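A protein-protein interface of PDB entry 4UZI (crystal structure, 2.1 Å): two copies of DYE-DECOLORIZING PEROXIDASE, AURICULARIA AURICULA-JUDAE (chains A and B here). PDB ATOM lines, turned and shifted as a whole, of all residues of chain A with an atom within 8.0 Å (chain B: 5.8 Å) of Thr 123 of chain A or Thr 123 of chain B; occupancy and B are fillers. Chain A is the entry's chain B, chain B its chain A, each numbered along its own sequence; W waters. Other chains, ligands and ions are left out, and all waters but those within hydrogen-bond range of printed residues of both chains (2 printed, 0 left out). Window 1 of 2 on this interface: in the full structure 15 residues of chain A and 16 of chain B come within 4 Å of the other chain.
The side-chain carboxylate of Asp 124 of chain A lies within salt-bridge range of the side-chain amino group of Lys 19 of chain B (2.8 Å).
OG1 of Thr 123 of chain B lies within hydrogen-bond range of OG1 of Thr 123 of chain A (3.1 Å).
The side-chain carboxylate (OD2) of Asp 124 of chain B lies within salt-bridge range of the side-chain amino group (NZ) of Lys 19 of chain A, 2.4 Å away.
The backbone carbonyl oxygen (O) of Ser 120 of chain B sits at hydrogen-bond distance from the backbone NH (N) of Lys 19 of chain B (2.7 Å).
The side-chain hydroxyl of Thr 122 of chain B lies close to the backbone NH of Asp 124 of chain B, at 3.4 Å.
The backbone carbonyl oxygen of Ser 120 of chain A lies within hydrogen-bond range of the backbone NH of Lys 19 of chain A (2.7 Å).
Thr 123 of chain A touches just one residue of chain B: Thr 123.
Of the printed residues of chain A, Lys 19 of chain B touches Asp 124.
Thr 123 of chain B touches just one residue of chain A: Thr 123 (3.1 Å).
Of the printed residues of chain A, Asp 124 of chain B touches Lys 19.
Of the 19 printed residues of chain A, 3 touch a printed residue of chain B.
Printed residues of chain B that touch a printed residue of chain A: Lys 19, Thr 123 and Asp 124.
Along chain B the printed residues that touch a printed residue of chain A span positions 19 to 124.
Lys 19 of chain A touches Asp 124 of chain B, and with the chains exchanged Asp 124 of chain A touches Lys 19 of chain B.
Thr 123 of chain A touches its own counterpart, Thr 123 of chain B.
Water W2 lies within hydrogen-bond range of the side-chain hydroxyl (OG1) of Thr 123 of chain A, the side-chain carboxylate (OD1) of Asp 124 of chain B and the side-chain hydroxyl (OG1) of Thr 123 of chain B.
Water W1 lies within hydrogen-bond range of the side-chain carboxylate (OD1) of Asp 124 of chain B and the side-chain amino group (NZ) of Lys 19 of chain A.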
ATOM      1  N   GLN A  18      -7.832  24.135   3.193  1.00  0.00           N
ATOM      2  CA  GLN A  18      -8.261  22.794   2.837  1.00  0.00           C
ATOM      3  C   GLN A  18      -7.919  21.821   3.962  1.00  0.00           C
ATOM      4  O   GLN A  18      -8.694  20.911   4.278  1.00  0.00           O
ATOM      5  CB  GLN A  18      -7.555  22.372   1.547  1.00  0.00           C
ATOM      6  CG  GLN A  18      -8.268  21.295   0.754  1.00  0.00           C
ATOM      7  CD  GLN A  18      -9.592  21.760   0.183  1.00  0.00           C
ATOM      8  OE1 GLN A  18     -10.019  22.896   0.394  1.00  0.00           O
ATOM      9  NE2 GLN A  18     -10.248  20.877  -0.553  1.00  0.00           N
ATOM     10  N   LYS A  19      -6.748  22.011   4.562  1.00  0.00           N
ATOM     11  CA  LYS A  19      -6.266  21.103   5.598  1.00  0.00           C
ATOM     12  C   LYS A  19      -6.096  21.837   6.920  1.00  0.00           C
ATOM     13  O   LYS A  19      -5.810  23.033   6.939  1.00  0.00           O
ATOM     14  CB  LYS A  19      -4.934  20.472   5.188  1.00  0.00           C
ATOM     15  CG  LYS A  19      -4.882  20.000   3.741  1.00  0.00           C
ATOM     16  CD  LYS A  19      -5.852  18.859   3.508  1.00  0.00           C
ATOM     17  CE  LYS A  19      -5.883  18.460   2.044  1.00  0.00           C
ATOM     18  NZ  LYS A  19      -6.310  17.042   1.917  1.00  0.00           N
ATOM     19  N   GLN A  20      -6.268  21.117   8.024  1.00  0.00           N
ATOM     20  CA  GLN A  20      -5.938  21.654   9.336  1.00  0.00           C
ATOM     21  C   GLN A  20      -5.236  20.626  10.208  1.00  0.00           C
ATOM     22  O   GLN A  20      -5.420  19.421  10.038  1.00  0.00           O
ATOM     23  CB  GLN A  20      -7.191  22.172  10.043  1.00  0.00           C
ATOM     24  CG  GLN A  20      -7.608  23.561   9.599  1.00  0.00           C
ATOM     25  CD  GLN A  20      -8.806  24.084  10.361  1.00  0.00           C
ATOM     26  OE1 GLN A  20      -8.943  23.852  11.560  1.00  0.00           O
ATOM     27  NE2 GLN A  20      -9.662  24.825   9.674  1.00  0.00           N
ATOM     28  N   LEU A  21      -4.435  21.109  11.151  1.00  0.00           N
ATOM     29  CA  LEU A  21      -3.885  20.247  12.185  1.00  0.00           C
ATOM     30  C   LEU A  21      -4.183  20.811  13.564  1.00  0.00           C
ATOM     31  O   LEU A  21      -4.033  22.006  13.793  1.00  0.00           O
ATOM     32  CB  LEU A  21      -2.375  20.084  12.005  1.00  0.00           C
ATOM     33  CG  LEU A  21      -1.675  19.267  13.096  1.00  0.00           C
ATOM     34  CD1 LEU A  21      -1.961  17.780  12.925  1.00  0.00           C
ATOM     35  CD2 LEU A  21      -0.173  19.531  13.086  1.00  0.00           C
ATOM     36  N   VAL A  60       0.557  29.095   5.610  1.00  0.00           N
ATOM     37  CA  VAL A  60       0.055  28.339   6.746  1.00  0.00           C
ATOM     38  C   VAL A  60      -0.529  29.315   7.764  1.00  0.00           C
ATOM     39  O   VAL A  60       0.180  30.182   8.283  1.00  0.00           O
ATOM     40  CB  VAL A  60       1.179  27.525   7.422  1.00  0.00           C
ATOM     41  CG1 VAL A  60       0.622  26.701   8.577  1.00  0.00           C
ATOM     42  CG2 VAL A  60       1.883  26.634   6.403  1.00  0.00           C
ATOM     43  N   SER A 120      -3.698  25.011   6.140  1.00  0.00           N
ATOM     44  CA  SER A 120      -3.032  25.232   4.873  1.00  0.00           C
ATOM     45  C   SER A 120      -3.717  24.396   3.805  1.00  0.00           C
ATOM     46  O   SER A 120      -4.531  23.525   4.112  1.00  0.00           O
ATOM     47  CB  SER A 120      -1.557  24.843   4.976  1.00  0.00           C
ATOM     48  OG  SER A 120      -0.884  25.110   3.764  1.00  0.00           O
ATOM     49  N   ASP A 121      -3.375  24.644   2.550  1.00  0.00           N
ATOM     50  CA  ASP A 121      -4.033  23.936   1.468  1.00  0.00           C
ATOM     51  C   ASP A 121      -3.373  22.607   1.115  1.00  0.00           C
ATOM     52  O   ASP A 121      -3.980  21.773   0.440  1.00  0.00           O
ATOM     53  CB  ASP A 121      -4.221  24.842   0.250  1.00  0.00           C
ATOM     54  CG  ASP A 121      -5.432  25.766   0.396  1.00  0.00           C
ATOM     55  OD1 ASP A 121      -6.363  25.410   1.152  1.00  0.00           O
ATOM     56  OD2 ASP A 121      -5.449  26.847  -0.229  1.00  0.00           O
ATOM     57  N   THR A 122      -2.177  22.373   1.654  1.00  0.00           N
ATOM     58  CA  THR A 122      -1.545  21.048   1.598  1.00  0.00           C
ATOM     59  C   THR A 122      -1.056  20.597   2.974  1.00  0.00           C
ATOM     60  O   THR A 122      -0.596  21.411   3.778  1.00  0.00           O
ATOM     61  CB  THR A 122      -0.343  21.018   0.635  1.00  0.00           C
ATOM     62  OG1 THR A 122       0.764  21.707   1.235  1.00  0.00           O
ATOM     63  CG2 THR A 122      -0.696  21.678  -0.695  1.00  0.00           C
ATOM     64  N   THR A 123      -1.091  19.289   3.212  1.00  0.00           N
ATOM     65  CA  THR A 123      -0.548  18.731   4.444  1.00  0.00           C
ATOM     66  C   THR A 123       0.975  18.860   4.481  1.00  0.00           C
ATOM     67  O   THR A 123       1.568  18.979   5.547  1.00  0.00           O
ATOM     68  CB  THR A 123      -0.955  17.259   4.634  1.00  0.00           C
ATOM     69  OG1 THR A 123      -0.562  16.503   3.483  1.00  0.00           O
ATOM     70  CG2 THR A 123      -2.469  17.150   4.809  1.00  0.00           C
ATOM     71  N   ASP A 124       1.597  18.904   3.306  1.00  0.00           N
ATOM     72  CA  ASP A 124       3.040  19.115   3.214  1.00  0.00           C
ATOM     73  C   ASP A 124       3.464  20.371   3.964  1.00  0.00           C
ATOM     74  O   ASP A 124       4.403  20.338   4.762  1.00  0.00           O
ATOM     75  CB  ASP A 124       3.462  19.238   1.754  1.00  0.00           C
ATOM     76  CG  ASP A 124       3.585  17.898   1.072  1.00  0.00           C
ATOM     77  OD1 ASP A 124       3.402  16.866   1.753  1.00  0.00           O
ATOM     78  OD2 ASP A 124       3.873  17.878  -0.143  1.00  0.00           O
ATOM     79  N   LEU A 125       2.814  21.488   3.640  1.00  0.00           N
ATOM     80  CA  LEU A 125       3.113  22.776   4.257  1.00  0.00           C
ATOM     81  C   LEU A 125       2.891  22.731   5.765  1.00  0.00           C
ATOM     82  O   LEU A 125       3.660  23.308   6.535  1.00  0.00           O
ATOM     83  CB  LEU A 125       2.242  23.873   3.647  1.00  0.00           C
ATOM     84  CG  LEU A 125       2.682  24.427   2.288  1.00  0.00           C
ATOM     85  CD1 LEU A 125       1.609  25.341   1.720  1.00  0.00           C
ATOM     86  CD2 LEU A 125       4.004  25.173   2.412  1.00  0.00           C
ATOM     87  N   ILE A 126       1.811  22.076   6.177  1.00  0.00           N
ATOM     88  CA  ILE A 126       1.513  21.930   7.589  1.00  0.00           C
ATOM     89  C   ILE A 126       2.658  21.218   8.308  1.00  0.00           C
ATOM     90  O   ILE A 126       3.082  21.650   9.372  1.00  0.00           O
ATOM     91  CB  ILE A 126       0.188  21.174   7.815  1.00  0.00           C
ATOM     92  CG1 ILE A 126      -1.001  22.115   7.605  1.00  0.00           C
ATOM     93  CG2 ILE A 126       0.147  20.581   9.219  1.00  0.00           C
ATOM     94  CD1 ILE A 126      -2.345  21.416   7.585  1.00  0.00           C
ATOM     95  N   ASP A 127       3.192  20.164   7.694  1.00  0.00           N
ATOM     96  CA  ASP A 127       4.245  19.368   8.321  1.00  0.00           C
ATOM     97  C   ASP A 127       5.562  20.143   8.444  1.00  0.00           C
ATOM     98  O   ASP A 127       6.314  19.969   9.399  1.00  0.00           O
ATOM     99  CB  ASP A 127       4.478  18.078   7.536  1.00  0.00           C
ATOM    100  CG  ASP A 127       3.312  17.106   7.647  1.00  0.00           C
ATOM    101  OD1 ASP A 127       2.450  17.296   8.531  1.00  0.00           O
ATOM    102  OD2 ASP A 127       3.267  16.147   6.849  1.00  0.00           O
ATOM    103  N   GLN A 128       5.859  20.961   7.447  1.00  0.00           N
ATOM    104  CA  GLN A 128       7.043  21.796   7.501  1.00  0.00           C
ATOM    105  C   GLN A 128       6.894  22.807   8.639  1.00  0.00           C
ATOM    106  O   GLN A 128       7.846  23.061   9.376  1.00  0.00           O
ATOM    107  CB  GLN A 128       7.274  22.493   6.157  1.00  0.00           C
ATOM    108  CG  GLN A 128       8.650  23.125   6.010  1.00  0.00           C
ATOM    109  CD  GLN A 128       9.768  22.123   6.217  1.00  0.00           C
ATOM    110  OE1 GLN A 128       9.749  21.034   5.648  1.00  0.00           O
ATOM    111  NE2 GLN A 128      10.735  22.476   7.055  1.00  0.00           N
ATOM    112  N   GLN A 129       5.674  23.296   8.852  1.00  0.00           N
ATOM    113  CA  GLN A 129       5.430  24.263   9.924  1.00  0.00           C
ATOM    114  C   GLN A 129       5.534  23.636  11.311  1.00  0.00           C
ATOM    115  O   GLN A 129       6.108  24.228  12.224  1.00  0.00           O
ATOM    116  CB  GLN A 129       4.086  24.975   9.752  1.00  0.00           C
ATOM    117  CG  GLN A 129       3.880  26.136  10.716  1.00  0.00           C
ATOM    118  CD  GLN A 129       4.716  27.350  10.353  1.00  0.00           C
ATOM    119  OE1 GLN A 129       5.666  27.699  11.054  1.00  0.00           O
ATOM    120  NE2 GLN A 129       4.383  27.984   9.233  1.00  0.00           N
ATOM    121  N   VAL A 130       5.012  22.425  11.460  1.00  0.00           N
ATOM    122  CA  VAL A 130       5.232  21.656  12.679  1.00  0.00           C
ATOM    123  C   VAL A 130       6.731  21.525  12.970  1.00  0.00           C
ATOM    124  O   VAL A 130       7.194  21.849  14.073  1.00  0.00           O
ATOM    125  CB  VAL A 130       4.585  20.262  12.593  1.00  0.00           C
ATOM    126  CG1 VAL A 130       5.069  19.379  13.730  1.00  0.00           C
ATOM    127  CG2 VAL A 130       3.064  20.380  12.613  1.00  0.00           C
ATOM    128  N   SER A 148      -5.209  15.421  12.541  1.00  0.00           N
ATOM    129  CA  SER A 148      -5.296  16.026  11.220  1.00  0.00           C
ATOM    130  C   SER A 148      -6.736  16.041  10.724  1.00  0.00           C
ATOM    131  O   SER A 148      -7.532  15.137  11.022  1.00  0.00           O
ATOM    132  CB  SER A 148      -4.417  15.273  10.226  1.00  0.00           C
ATOM    133  OG  SER A 148      -3.073  15.248  10.663  1.00  0.00           O
ATOM    134  N   ALA A 149      -7.069  17.076   9.967  1.00  0.00           N
ATOM    135  CA  ALA A 149      -8.428  17.257   9.483  1.00  0.00           C
ATOM    136  C   ALA A 149      -8.344  17.817   8.077  1.00  0.00           C
ATOM    137  O   ALA A 149      -7.317  18.368   7.687  1.00  0.00           O
ATOM    138  CB  ALA A 149      -9.189  18.205  10.398  1.00  0.00           C
ATOM    139  N   SER A 150      -9.378  17.584   7.280  1.00  0.00           N
ATOM    140  CA  SER A 150      -9.475  18.247   5.989  1.00  0.00           C
ATOM    141  C   SER A 150     -10.901  18.406   5.490  1.00  0.00           C
ATOM    142  O   SER A 150     -11.807  17.683   5.906  1.00  0.00           O
ATOM    143  CB  SER A 150      -8.606  17.551   4.939  1.00  0.00           C
ATOM    144  OG  SER A 150      -9.093  16.265   4.639  1.00  0.00           O
ATOM    145  N   LYS B  19       5.659  11.002  -3.741  1.00  0.00           N
ATOM    146  CA  LYS B  19       5.566  10.544  -2.364  1.00  0.00           C
ATOM    147  C   LYS B  19       5.622   9.022  -2.289  1.00  0.00           C
ATOM    148  O   LYS B  19       5.078   8.327  -3.147  1.00  0.00           O
ATOM    149  CB  LYS B  19       4.260  11.028  -1.726  1.00  0.00           C
ATOM    150  CG  LYS B  19       3.926  12.488  -1.977  1.00  0.00           C
ATOM    151  CD  LYS B  19       4.901  13.419  -1.269  1.00  0.00           C
ATOM    152  CE  LYS B  19       4.443  14.866  -1.375  1.00  0.00           C
ATOM    153  NZ  LYS B  19       5.557  15.819  -1.115  1.00  0.00           N
ATOM    154  N   SER B 120       2.639   7.751  -4.691  1.00  0.00           N
ATOM    155  CA  SER B 120       1.643   8.612  -5.307  1.00  0.00           C
ATOM    156  C   SER B 120       2.210  10.017  -5.357  1.00  0.00           C
ATOM    157  O   SER B 120       3.210  10.305  -4.705  1.00  0.00           O
ATOM    158  CB  SER B 120       0.360   8.602  -4.476  1.00  0.00           C
ATOM    159  OG  SER B 120      -0.757   8.935  -5.275  1.00  0.00           O
ATOM    160  N   ASP B 121       1.544  10.908  -6.084  1.00  0.00           N
ATOM    161  CA  ASP B 121       2.008  12.285  -6.178  1.00  0.00           C
ATOM    162  C   ASP B 121       1.504  13.160  -5.026  1.00  0.00           C
ATOM    163  O   ASP B 121       2.028  14.251  -4.789  1.00  0.00           O
ATOM    164  CB  ASP B 121       1.660  12.886  -7.542  1.00  0.00           C
ATOM    165  CG  ASP B 121       2.532  12.327  -8.661  1.00  0.00           C
ATOM    166  OD1 ASP B 121       3.688  11.931  -8.385  1.00  0.00           O
ATOM    167  OD2 ASP B 121       2.067  12.290  -9.818  1.00  0.00           O
ATOM    168  N   THR B 122       0.526  12.659  -4.278  1.00  0.00           N
ATOM    169  CA  THR B 122       0.126  13.298  -3.031  1.00  0.00           C
ATOM    170  C   THR B 122       0.077  12.296  -1.883  1.00  0.00           C
ATOM    171  O   THR B 122      -0.117  11.102  -2.098  1.00  0.00           O
ATOM    172  CB  THR B 122      -1.251  13.975  -3.153  1.00  0.00           C
ATOM    173  OG1 THR B 122      -2.286  12.985  -3.059  1.00  0.00           O
ATOM    174  CG2 THR B 122      -1.370  14.709  -4.478  1.00  0.00           C
ATOM    175  N   THR B 123       0.185  12.797  -0.659  1.00  0.00           N
ATOM    176  CA  THR B 123       0.054  11.949   0.518  1.00  0.00           C
ATOM    177  C   THR B 123      -1.414  11.640   0.826  1.00  0.00           C
ATOM    178  O   THR B 123      -1.720  10.604   1.410  1.00  0.00           O
ATOM    179  CB  THR B 123       0.756  12.568   1.746  1.00  0.00           C
ATOM    180  OG1 THR B 123       0.138  13.817   2.077  1.00  0.00           O
ATOM    181  CG2 THR B 123       2.228  12.820   1.437  1.00  0.00           C
ATOM    182  N   ASP B 124      -2.320  12.497   0.354  1.00  0.00           N
ATOM    183  CA  ASP B 124      -3.764  12.255   0.481  1.00  0.00           C
ATOM    184  C   ASP B 124      -4.150  10.915  -0.147  1.00  0.00           C
ATOM    185  O   ASP B 124      -4.828  10.090   0.470  1.00  0.00           O
ATOM    186  CB  ASP B 124      -4.563  13.381  -0.191  1.00  0.00           C
ATOM    187  CG  ASP B 124      -4.770  14.583   0.718  1.00  0.00           C
ATOM    188  OD1 ASP B 124      -4.342  14.536   1.891  1.00  0.00           O
ATOM    189  OD2 ASP B 124      -5.374  15.575   0.261  1.00  0.00           O
ATOM    190  N   LEU B 125      -3.688  10.705  -1.372  1.00  0.00           N
ATOM    191  CA  LEU B 125      -3.967   9.484  -2.116  1.00  0.00           C
ATOM    192  C   LEU B 125      -3.409   8.250  -1.421  1.00  0.00           C
ATOM    193  O   LEU B 125      -4.027   7.184  -1.431  1.00  0.00           O
ATOM    194  CB  LEU B 125      -3.388   9.593  -3.527  1.00  0.00           C
ATOM    195  CG  LEU B 125      -4.175  10.493  -4.476  1.00  0.00           C
ATOM    196  CD1 LEU B 125      -3.415  10.691  -5.778  1.00  0.00           C
ATOM    197  CD2 LEU B 125      -5.559   9.911  -4.733  1.00  0.00           C
ATOM    198  N   ILE B 126      -2.224   8.393  -0.838  1.00  0.00           N
ATOM    199  CA  ILE B 126      -1.611   7.304  -0.091  1.00  0.00           C
ATOM    200  C   ILE B 126      -2.418   6.968   1.157  1.00  0.00           C
ATOM    201  O   ILE B 126      -2.694   5.801   1.420  1.00  0.00           O
ATOM    202  CB  ILE B 126      -0.161   7.636   0.305  1.00  0.00           C
ATOM    203  CG1 ILE B 126       0.751   7.542  -0.920  1.00  0.00           C
ATOM    204  CG2 ILE B 126       0.315   6.715   1.427  1.00  0.00           C
ATOM    205  CD1 ILE B 126       2.177   7.971  -0.652  1.00  0.00           C
ATOM    206  N   ASP B 127      -2.792   8.001   1.913  1.00  0.00           N
ATOM    207  CA  ASP B 127      -3.621   7.861   3.110  1.00  0.00           C
ATOM    208  C   ASP B 127      -4.924   7.106   2.839  1.00  0.00           C
ATOM    209  O   ASP B 127      -5.363   6.284   3.644  1.00  0.00           O
ATOM    210  CB  ASP B 127      -3.971   9.243   3.673  1.00  0.00           C
ATOM    211  CG  ASP B 127      -2.819   9.882   4.431  1.00  0.00           C
ATOM    212  OD1 ASP B 127      -1.890   9.160   4.852  1.00  0.00           O
ATOM    213  OD2 ASP B 127      -2.874  11.110   4.645  1.00  0.00           O
ATOM    214  N   GLN B 128      -5.589   7.455   1.750  1.00  0.00           N
ATOM    215  CA  GLN B 128      -6.859   6.825   1.429  1.00  0.00           C
ATOM    216  C   GLN B 128      -6.619   5.365   1.038  1.00  0.00           C
ATOM    217  O   GLN B 128      -7.455   4.497   1.288  1.00  0.00           O
ATOM    218  CB  GLN B 128      -7.571   7.587   0.306  1.00  0.00           C
ATOM    219  CG  GLN B 128      -8.984   7.097   0.018  1.00  0.00           C
ATOM    220  CD  GLN B 128      -9.888   7.183   1.234  1.00  0.00           C
ATOM    221  OE1 GLN B 128      -9.938   8.212   1.916  1.00  0.00           O
ATOM    222  NE2 GLN B 128     -10.581   6.088   1.536  1.00  0.00           N
HETATM  223  O   HOH W   1      -5.641  15.257   4.137  1.00  0.00           O
HETATM  224  O   HOH W   2      -2.061  14.822   2.648  1.00  0.00           O
